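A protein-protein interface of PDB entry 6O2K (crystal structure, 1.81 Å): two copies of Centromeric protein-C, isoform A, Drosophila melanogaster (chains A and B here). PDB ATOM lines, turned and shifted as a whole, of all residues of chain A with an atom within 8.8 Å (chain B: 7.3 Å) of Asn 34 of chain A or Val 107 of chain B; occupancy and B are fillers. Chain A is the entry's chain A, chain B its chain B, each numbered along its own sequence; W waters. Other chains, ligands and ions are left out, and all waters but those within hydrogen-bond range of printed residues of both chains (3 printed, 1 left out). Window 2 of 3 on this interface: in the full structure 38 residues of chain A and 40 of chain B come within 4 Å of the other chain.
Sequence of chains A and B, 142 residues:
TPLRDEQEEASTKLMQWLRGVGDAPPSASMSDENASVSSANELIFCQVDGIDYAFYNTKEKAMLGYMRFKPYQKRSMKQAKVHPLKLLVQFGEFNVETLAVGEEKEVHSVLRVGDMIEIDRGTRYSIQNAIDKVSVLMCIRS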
ATOM      1  N   ASP A  32     -27.863  25.297  -3.325  1.00  0.00           N
ATOM      2  CA  ASP A  32     -27.655  23.907  -3.733  1.00  0.00           C
ATOM      3  C   ASP A  32     -27.317  23.843  -5.213  1.00  0.00           C
ATOM      4  O   ASP A  32     -28.076  24.338  -6.048  1.00  0.00           O
ATOM      5  CB  ASP A  32     -28.900  23.055  -3.440  1.00  0.00           C
ATOM      6  CG  ASP A  32     -28.697  21.578  -3.769  1.00  0.00           C
ATOM      7  OD1 ASP A  32     -28.660  20.748  -2.828  1.00  0.00           O
ATOM      8  OD2 ASP A  32     -28.586  21.237  -4.967  1.00  0.00           O
ATOM      9  N   GLU A  33     -26.179  23.225  -5.537  1.00  0.00           N
ATOM     10  CA  GLU A  33     -25.725  23.079  -6.915  1.00  0.00           C
ATOM     11  C   GLU A  33     -25.587  21.617  -7.321  1.00  0.00           C
ATOM     12  O   GLU A  33     -24.883  21.309  -8.284  1.00  0.00           O
ATOM     13  CB  GLU A  33     -24.380  23.774  -7.111  1.00  0.00           C
ATOM     14  CG  GLU A  33     -24.447  25.268  -7.190  1.00  0.00           C
ATOM     15  CD  GLU A  33     -23.196  25.828  -7.821  1.00  0.00           C
ATOM     16  OE1 GLU A  33     -23.299  26.332  -8.964  1.00  0.00           O
ATOM     17  OE2 GLU A  33     -22.115  25.718  -7.182  1.00  0.00           O
ATOM     18  N   ASN A  34     -26.194  20.706  -6.577  1.00  0.00           N
ATOM     19  CA  ASN A  34     -26.067  19.281  -6.865  1.00  0.00           C
ATOM     20  C   ASN A  34     -26.830  18.948  -8.139  1.00  0.00           C
ATOM     21  O   ASN A  34     -28.043  19.163  -8.206  1.00  0.00           O
ATOM     22  CB  ASN A  34     -26.616  18.480  -5.686  1.00  0.00           C
ATOM     23  CG  ASN A  34     -26.325  17.001  -5.784  1.00  0.00           C
ATOM     24  OD1 ASN A  34     -25.865  16.502  -6.816  1.00  0.00           O
ATOM     25  ND2 ASN A  34     -26.619  16.279  -4.705  1.00  0.00           N
ATOM     26  N   ALA A  35     -26.131  18.418  -9.151  1.00  0.00           N
ATOM     27  CA  ALA A  35     -26.823  18.056 -10.386  1.00  0.00           C
ATOM     28  C   ALA A  35     -27.845  16.950 -10.167  1.00  0.00           C
ATOM     29  O   ALA A  35     -28.794  16.829 -10.949  1.00  0.00           O
ATOM     30  CB  ALA A  35     -25.831  17.616 -11.460  1.00  0.00           C
ATOM     31  N   SER A  36     -27.649  16.114  -9.143  1.00  0.00           N
ATOM     32  CA  SER A  36     -28.571  15.011  -8.899  1.00  0.00           C
ATOM     33  C   SER A  36     -29.927  15.503  -8.396  1.00  0.00           C
ATOM     34  O   SER A  36     -30.929  14.805  -8.564  1.00  0.00           O
ATOM     35  CB  SER A  36     -27.976  14.032  -7.881  1.00  0.00           C
ATOM     36  OG  SER A  36     -26.650  13.640  -8.262  1.00  0.00           O
ATOM     37  N   VAL A  37     -29.970  16.678  -7.775  1.00  0.00           N
ATOM     38  CA  VAL A  37     -31.195  17.236  -7.198  1.00  0.00           C
ATOM     39  C   VAL A  37     -31.934  18.038  -8.260  1.00  0.00           C
ATOM     40  O   VAL A  37     -31.328  18.852  -8.967  1.00  0.00           O
ATOM     41  CB  VAL A  37     -30.881  18.120  -5.975  1.00  0.00           C
ATOM     42  CG1 VAL A  37     -32.143  18.858  -5.523  1.00  0.00           C
ATOM     43  CG2 VAL A  37     -30.340  17.271  -4.814  1.00  0.00           C
ATOM     44  N   SER A  38     -33.246  17.819  -8.366  1.00  0.00           N
ATOM     45  CA  SER A  38     -34.122  18.688  -9.140  1.00  0.00           C
ATOM     46  C   SER A  38     -35.230  19.176  -8.214  1.00  0.00           C
ATOM     47  O   SER A  38     -36.059  18.378  -7.753  1.00  0.00           O
ATOM     48  CB  SER A  38     -34.702  17.960 -10.354  1.00  0.00           C
ATOM     49  OG  SER A  38     -35.396  18.876 -11.192  1.00  0.00           O
ATOM     50  N   SER A  39     -35.250  20.479  -7.951  1.00  0.00           N
ATOM     51  CA  SER A  39     -36.159  21.041  -6.962  1.00  0.00           C
ATOM     52  C   SER A  39     -37.529  21.287  -7.584  1.00  0.00           C
ATOM     53  O   SER A  39     -37.661  21.445  -8.797  1.00  0.00           O
ATOM     54  CB  SER A  39     -35.585  22.345  -6.406  1.00  0.00           C
ATOM     55  OG  SER A  39     -34.569  22.058  -5.462  1.00  0.00           O
ATOM     56  N   GLU A  42     -37.979  24.177  -9.834  1.00  0.00           N
ATOM     57  CA  GLU A  42     -37.473  24.075 -11.199  1.00  0.00           C
ATOM     58  C   GLU A  42     -38.536  23.678 -12.209  1.00  0.00           C
ATOM     59  O   GLU A  42     -38.249  23.672 -13.411  1.00  0.00           O
ATOM     60  CB  GLU A  42     -36.348  23.032 -11.293  1.00  0.00           C
ATOM     61  CG  GLU A  42     -34.960  23.469 -10.863  1.00  0.00           C
ATOM     62  CD  GLU A  42     -34.027  22.274 -10.675  1.00  0.00           C
ATOM     63  OE1 GLU A  42     -33.984  21.377 -11.566  1.00  0.00           O
ATOM     64  OE2 GLU A  42     -33.352  22.213  -9.618  1.00  0.00           O
ATOM     65  N   ASN A  57     -35.589  17.962 -13.998  1.00  0.00           N
ATOM     66  CA  ASN A  57     -34.298  17.770 -14.650  1.00  0.00           C
ATOM     67  C   ASN A  57     -33.705  16.433 -14.213  1.00  0.00           C
ATOM     68  O   ASN A  57     -33.350  16.251 -13.042  1.00  0.00           O
ATOM     69  CB  ASN A  57     -33.351  18.909 -14.305  1.00  0.00           C
ATOM     70  CG  ASN A  57     -31.957  18.652 -14.818  1.00  0.00           C
ATOM     71  OD1 ASN A  57     -31.130  18.018 -14.147  1.00  0.00           O
ATOM     72  ND2 ASN A  57     -31.695  19.108 -16.027  1.00  0.00           N
ATOM     73  N   VAL B  96     -30.398  13.897   2.736  1.00  0.00           N
ATOM     74  CA  VAL B  96     -29.871  12.760   1.985  1.00  0.00           C
ATOM     75  C   VAL B  96     -28.368  12.929   1.831  1.00  0.00           C
ATOM     76  O   VAL B  96     -27.905  13.989   1.400  1.00  0.00           O
ATOM     77  CB  VAL B  96     -30.545  12.631   0.606  1.00  0.00           C
ATOM     78  CG1 VAL B  96     -29.951  11.444  -0.176  1.00  0.00           C
ATOM     79  CG2 VAL B  96     -32.076  12.499   0.760  1.00  0.00           C
ATOM     80  N   GLU B  97     -27.612  11.883   2.173  1.00  0.00           N
ATOM     81  CA  GLU B  97     -26.163  11.864   1.992  1.00  0.00           C
ATOM     82  C   GLU B  97     -25.823  10.872   0.892  1.00  0.00           C
ATOM     83  O   GLU B  97     -26.291   9.729   0.932  1.00  0.00           O
ATOM     84  CB  GLU B  97     -25.434  11.470   3.284  1.00  0.00           C
ATOM     85  CG  GLU B  97     -26.040  12.015   4.583  1.00  0.00           C
ATOM     86  CD  GLU B  97     -25.987  13.536   4.693  1.00  0.00           C
ATOM     87  OE1 GLU B  97     -27.024  14.141   5.066  1.00  0.00           O
ATOM     88  OE2 GLU B  97     -24.919  14.125   4.410  1.00  0.00           O
ATOM     89  N   THR B  98     -25.012  11.307  -0.091  1.00  0.00           N
ATOM     90  CA  THR B  98     -24.656  10.458  -1.226  1.00  0.00           C
ATOM     91  C   THR B  98     -23.151  10.442  -1.441  1.00  0.00           C
ATOM     92  O   THR B  98     -22.483  11.464  -1.263  1.00  0.00           O
ATOM     93  CB  THR B  98     -25.330  10.911  -2.542  1.00  0.00           C
ATOM     94  OG1 THR B  98     -25.056  12.297  -2.782  1.00  0.00           O
ATOM     95  CG2 THR B  98     -26.842  10.697  -2.480  1.00  0.00           C
ATOM     96  N   LEU B  99     -22.635   9.272  -1.838  1.00  0.00           N
ATOM     97  CA  LEU B  99     -21.251   9.075  -2.260  1.00  0.00           C
ATOM     98  C   LEU B  99     -21.293   8.304  -3.573  1.00  0.00           C
ATOM     99  O   LEU B  99     -21.686   7.130  -3.596  1.00  0.00           O
ATOM    100  CB  LEU B  99     -20.445   8.311  -1.204  1.00  0.00           C
ATOM    101  CG  LEU B  99     -19.021   7.933  -1.630  1.00  0.00           C
ATOM    102  CD1 LEU B  99     -18.189   9.169  -1.920  1.00  0.00           C
ATOM    103  CD2 LEU B  99     -18.353   7.049  -0.575  1.00  0.00           C
ATOM    104  N   ALA B 100     -20.912   8.961  -4.668  1.00  0.00           N
ATOM    105  CA  ALA B 100     -21.051   8.377  -5.997  1.00  0.00           C
ATOM    106  C   ALA B 100     -19.781   7.637  -6.389  1.00  0.00           C
ATOM    107  O   ALA B 100     -18.692   7.982  -5.937  1.00  0.00           O
ATOM    108  CB  ALA B 100     -21.353   9.460  -7.034  1.00  0.00           C
ATOM    109  N   GLU B 103     -16.020   9.036  -6.796  1.00  0.00           N
ATOM    110  CA  GLU B 103     -15.898  10.288  -6.068  1.00  0.00           C
ATOM    111  C   GLU B 103     -15.429  10.018  -4.644  1.00  0.00           C
ATOM    112  O   GLU B 103     -15.585   8.917  -4.107  1.00  0.00           O
ATOM    113  CB  GLU B 103     -17.234  11.052  -6.091  1.00  0.00           C
ATOM    114  CG  GLU B 103     -17.710  11.271  -7.527  1.00  0.00           C
ATOM    115  CD  GLU B 103     -18.909  12.189  -7.659  1.00  0.00           C
ATOM    116  OE1 GLU B 103     -19.257  12.901  -6.683  1.00  0.00           O
ATOM    117  OE2 GLU B 103     -19.506  12.191  -8.762  1.00  0.00           O
ATOM    118  N   GLU B 104     -14.824  11.042  -4.044  1.00  0.00           N
ATOM    119  CA  GLU B 104     -14.284  10.947  -2.696  1.00  0.00           C
ATOM    120  C   GLU B 104     -15.142  11.628  -1.645  1.00  0.00           C
ATOM    121  O   GLU B 104     -15.087  11.241  -0.477  1.00  0.00           O
ATOM    122  CB  GLU B 104     -12.879  11.566  -2.643  1.00  0.00           C
ATOM    123  CG  GLU B 104     -11.776  10.675  -3.179  1.00  0.00           C
ATOM    124  CD  GLU B 104     -10.421  11.012  -2.589  1.00  0.00           C
ATOM    125  OE1 GLU B 104      -9.400  10.794  -3.280  1.00  0.00           O
ATOM    126  OE2 GLU B 104     -10.377  11.499  -1.436  1.00  0.00           O
ATOM    127  N   LYS B 105     -15.924  12.633  -2.028  1.00  0.00           N
ATOM    128  CA  LYS B 105     -16.641  13.473  -1.080  1.00  0.00           C
ATOM    129  C   LYS B 105     -18.086  13.010  -0.956  1.00  0.00           C
ATOM    130  O   LYS B 105     -18.785  12.844  -1.965  1.00  0.00           O
ATOM    131  CB  LYS B 105     -16.588  14.942  -1.510  1.00  0.00           C
ATOM    132  CG  LYS B 105     -16.324  15.929  -0.377  1.00  0.00           C
ATOM    133  CD  LYS B 105     -14.840  16.245  -0.210  1.00  0.00           C
ATOM    134  CE  LYS B 105     -14.643  17.555   0.558  1.00  0.00           C
ATOM    135  NZ  LYS B 105     -13.360  17.595   1.320  1.00  0.00           N
ATOM    136  N   GLU B 106     -18.517  12.780   0.278  1.00  0.00           N
ATOM    137  CA  GLU B 106     -19.935  12.641   0.571  1.00  0.00           C
ATOM    138  C   GLU B 106     -20.614  13.999   0.429  1.00  0.00           C
ATOM    139  O   GLU B 106     -20.081  15.021   0.872  1.00  0.00           O
ATOM    140  CB  GLU B 106     -20.119  12.091   1.986  1.00  0.00           C
ATOM    141  CG  GLU B 106     -21.485  11.465   2.261  1.00  0.00           C
ATOM    142  CD  GLU B 106     -21.571  10.823   3.644  1.00  0.00           C
ATOM    143  OE1 GLU B 106     -22.412  11.265   4.458  1.00  0.00           O
ATOM    144  OE2 GLU B 106     -20.796   9.880   3.917  1.00  0.00           O
ATOM    145  N   VAL B 107     -21.787  14.018  -0.207  1.00  0.00           N
ATOM    146  CA  VAL B 107     -22.520  15.248  -0.475  1.00  0.00           C
ATOM    147  C   VAL B 107     -23.845  15.205   0.271  1.00  0.00           C
ATOM    148  O   VAL B 107     -24.534  14.177   0.280  1.00  0.00           O
ATOM    149  CB  VAL B 107     -22.740  15.461  -1.989  1.00  0.00           C
ATOM    150  CG1 VAL B 107     -23.646  16.653  -2.244  1.00  0.00           C
ATOM    151  CG2 VAL B 107     -21.371  15.647  -2.716  1.00  0.00           C
ATOM    152  N   HIS B 108     -24.196  16.334   0.884  1.00  0.00           N
ATOM    153  CA  HIS B 108     -25.375  16.483   1.720  1.00  0.00           C
ATOM    154  C   HIS B 108     -26.403  17.328   0.964  1.00  0.00           C
ATOM    155  O   HIS B 108     -26.080  18.424   0.493  1.00  0.00           O
ATOM    156  CB  HIS B 108     -24.974  17.137   3.051  1.00  0.00           C
ATOM    157  CG  HIS B 108     -26.125  17.607   3.887  1.00  0.00           C
ATOM    158  ND1 HIS B 108     -26.833  16.767   4.721  1.00  0.00           N
ATOM    159  CD2 HIS B 108     -26.676  18.836   4.038  1.00  0.00           C
ATOM    160  CE1 HIS B 108     -27.779  17.454   5.339  1.00  0.00           C
ATOM    161  NE2 HIS B 108     -27.706  18.712   4.942  1.00  0.00           N
ATOM    162  N   SER B 109     -27.630  16.814   0.826  1.00  0.00           N
ATOM    163  CA  SER B 109     -28.710  17.543   0.176  1.00  0.00           C
ATOM    164  C   SER B 109     -29.928  17.577   1.084  1.00  0.00           C
ATOM    165  O   SER B 109     -30.184  16.636   1.836  1.00  0.00           O
ATOM    166  CB  SER B 109     -29.105  16.926  -1.182  1.00  0.00           C
ATOM    167  OG  SER B 109     -27.977  16.542  -1.950  1.00  0.00           O
ATOM    168  N   MET B 116     -36.852  16.225  -5.721  1.00  0.00           N
ATOM    169  CA  MET B 116     -36.404  14.897  -6.122  1.00  0.00           C
ATOM    170  C   MET B 116     -34.878  14.835  -6.181  1.00  0.00           C
ATOM    171  O   MET B 116     -34.204  15.826  -6.488  1.00  0.00           O
ATOM    172  CB  MET B 116     -36.989  14.512  -7.500  1.00  0.00           C
ATOM    173  CG  MET B 116     -36.681  13.093  -7.938  1.00  0.00           C
ATOM    174  SD  MET B 116     -35.227  13.100  -9.024  1.00  0.00           S
ATOM    175  CE  MET B 116     -35.927  13.957 -10.406  1.00  0.00           C
ATOM    176  N   ILE B 117     -34.333  13.657  -5.884  1.00  0.00           N
ATOM    177  CA  ILE B 117     -32.918  13.384  -6.107  1.00  0.00           C
ATOM    178  C   ILE B 117     -32.778  12.079  -6.884  1.00  0.00           C
ATOM    179  O   ILE B 117     -33.512  11.117  -6.644  1.00  0.00           O
ATOM    180  CB  ILE B 117     -32.121  13.340  -4.780  1.00  0.00           C
ATOM    181  CG1 ILE B 117     -30.612  13.290  -5.067  1.00  0.00           C
ATOM    182  CG2 ILE B 117     -32.542  12.143  -3.922  1.00  0.00           C
ATOM    183  CD1 ILE B 117     -29.748  13.489  -3.809  1.00  0.00           C
ATOM    184  N   GLU B 118     -31.849  12.067  -7.838  1.00  0.00           N
ATOM    185  CA  GLU B 118     -31.522  10.905  -8.645  1.00  0.00           C
ATOM    186  C   GLU B 118     -30.313  10.214  -8.010  1.00  0.00           C
ATOM    187  O   GLU B 118     -29.284  10.857  -7.772  1.00  0.00           O
ATOM    188  CB  GLU B 118     -31.208  11.350 -10.086  1.00  0.00           C
ATOM    189  CG  GLU B 118     -31.367  10.299 -11.172  1.00  0.00           C
ATOM    190  CD  GLU B 118     -31.380  10.907 -12.589  1.00  0.00           C
ATOM    191  OE1 GLU B 118     -31.108  12.116 -12.747  1.00  0.00           O
ATOM    192  OE2 GLU B 118     -31.671  10.164 -13.544  1.00  0.00           O
ATOM    193  N   ARG B 124     -23.705   5.113  -2.857  1.00  0.00           N
ATOM    194  CA  ARG B 124     -24.058   4.805  -1.476  1.00  0.00           C
ATOM    195  C   ARG B 124     -24.825   5.991  -0.911  1.00  0.00           C
ATOM    196  O   ARG B 124     -24.362   7.133  -1.008  1.00  0.00           O
ATOM    197  CB  ARG B 124     -22.812   4.519  -0.637  1.00  0.00           C
ATOM    198  CG  ARG B 124     -22.134   3.212  -1.013  1.00  0.00           C
ATOM    199  CD  ARG B 124     -20.993   2.848  -0.066  1.00  0.00           C
ATOM    200  NE  ARG B 124     -20.228   1.728  -0.606  1.00  0.00           N
ATOM    201  CZ  ARG B 124     -20.587   0.451  -0.504  1.00  0.00           C
ATOM    202  NH1 ARG B 124     -19.826  -0.494  -1.042  1.00  0.00           N
ATOM    203  NH2 ARG B 124     -21.697   0.114   0.141  1.00  0.00           N
ATOM    204  N   SER B 126     -27.691   7.540   2.251  1.00  0.00           N
ATOM    205  CA  SER B 126     -28.452   7.437   3.491  1.00  0.00           C
ATOM    206  C   SER B 126     -29.476   8.567   3.564  1.00  0.00           C
ATOM    207  O   SER B 126     -29.320   9.616   2.928  1.00  0.00           O
ATOM    208  CB  SER B 126     -27.536   7.473   4.715  1.00  0.00           C
ATOM    209  OG  SER B 126     -27.023   8.778   4.895  1.00  0.00           O
HETATM  210  O   HOH W   1     -27.139  11.745 -10.125  1.00  0.00           O
HETATM  211  O   HOH W   2     -27.284  11.048  -6.089  1.00  0.00           O
HETATM  212  O   HOH W   3     -26.006  19.123  -2.318  1.00  0.00           O
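The backbone NH (N) of Ser 38 of chain A sits at hydrogen-bond distance from the backbone carbonyl oxygen (O) of Met 116 of chain B, 2.9 Å away.
O of Ser 36 of chain A is in hydrogen-bond range of N of Glu 118 of chain B, at 3.0 Å.
The side-chain amide nitrogen of Asn 34 of chain A lies within hydrogen-bond range of the side-chain hydroxyl of Ser 109 of chain B (3.1 Å).
The backbone NH (N) of Asn 57 of chain A sits at hydrogen-bond distance from the side-chain hydroxyl (OG) of Ser 38 of chain A (3.0 Å).
The side-chain carboxylate of Glu 42 of chain A sits at hydrogen-bond distance from the side-chain hydroxyl of Ser 38 of chain A (2.9 Å).
O of Thr 98 of chain B is in hydrogen-bond range of N of Val 107 of chain B (2.8 Å).
SD of Met 116 of chain B lies within hydrogen-bond range of N of Glu 118 of chain B, at 3.7 Å.
OD1 of Asn 34 of chain A lies within hydrogen-bond range of N of Ser 36 of chain A (3.0 Å).
The side-chain carboxylate (OD2) of Asp 32 of chain A sits at hydrogen-bond distance from the backbone NH (N) of Asn 34 of chain A (2.9 Å).
Among the printed residues, merely in contact across the chains: Val 37 of chain A with Met 116 of chain B, Ser 36 of chain A with Ile 117 of chain B, Val 37 of chain A with Ser 109 of chain B, Asn 34 of chain A with Val 107 of chain B and Val 37 of chain A with Ile 117 of chain B.
Asn 34 of chain A touches two residues of chain B.
Of the printed residues of chain B, Val 37 of chain A touches Ser 109 (3.8 Å), Met 116 (3.4 Å) and Ile 117 (3.96 Å).
Of the printed residues of chain B, Ser 38 of chain A touches Met 116 (2.9 Å).
Glu 97 of chain B touches none of the printed residues of chain A.
The nearest residue of chain A that does not touch Val 107 of chain B is Asp 32 of chain A (6.5 Å).
The nearest printed residue of chain A that does not touch Ser 109 of chain B is Asp 32 of chain A (4.2 Å).
Hydrophobic or aromatic side chains of chain B that line the printed part of chain A: Val 107, Met 116 and Ile 117.
Of the 10 printed residues of chain A, 4 touch a printed residue of chain B.
Printed residues of chain A that touch a printed residue of chain B: Asn 34, Ser 36, Val 37 and Ser 38.
Hydrophobic or aromatic side chains of chain A that line the printed part of chain B: Val 37.
Among the printed residues, 8 pairs touch across the chains.
Among the printed residues, no Asp or Glu carboxylate lies within 4 Å of a Lys or Arg side-chain nitrogen of the other chain.
No position is printed for both chains.
Of the 8 pairs that touch across the chains among the printed residues, none has its exchanged pair printed and touching as well.
Water W2 lies within hydrogen-bond range of the backbone carbonyl oxygen (O) of Glu 118 of chain B (2.6 Å) and the side-chain hydroxyl (OG) of Ser 36 of chain A (3.4 Å).
Water W1 lies within hydrogen-bond range of the side-chain hydroxyl of Ser 36 of chain A (2.7 Å) and the backbone carbonyl oxygen of Glu 118 of chain B (3.3 Å).
Water W3 lies within hydrogen-bond range of the backbone carbonyl oxygen of His 108 of chain B, the side-chain carboxylate of Asp 32 of chain A and the side-chain hydroxyl of Ser 109 of chain B.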
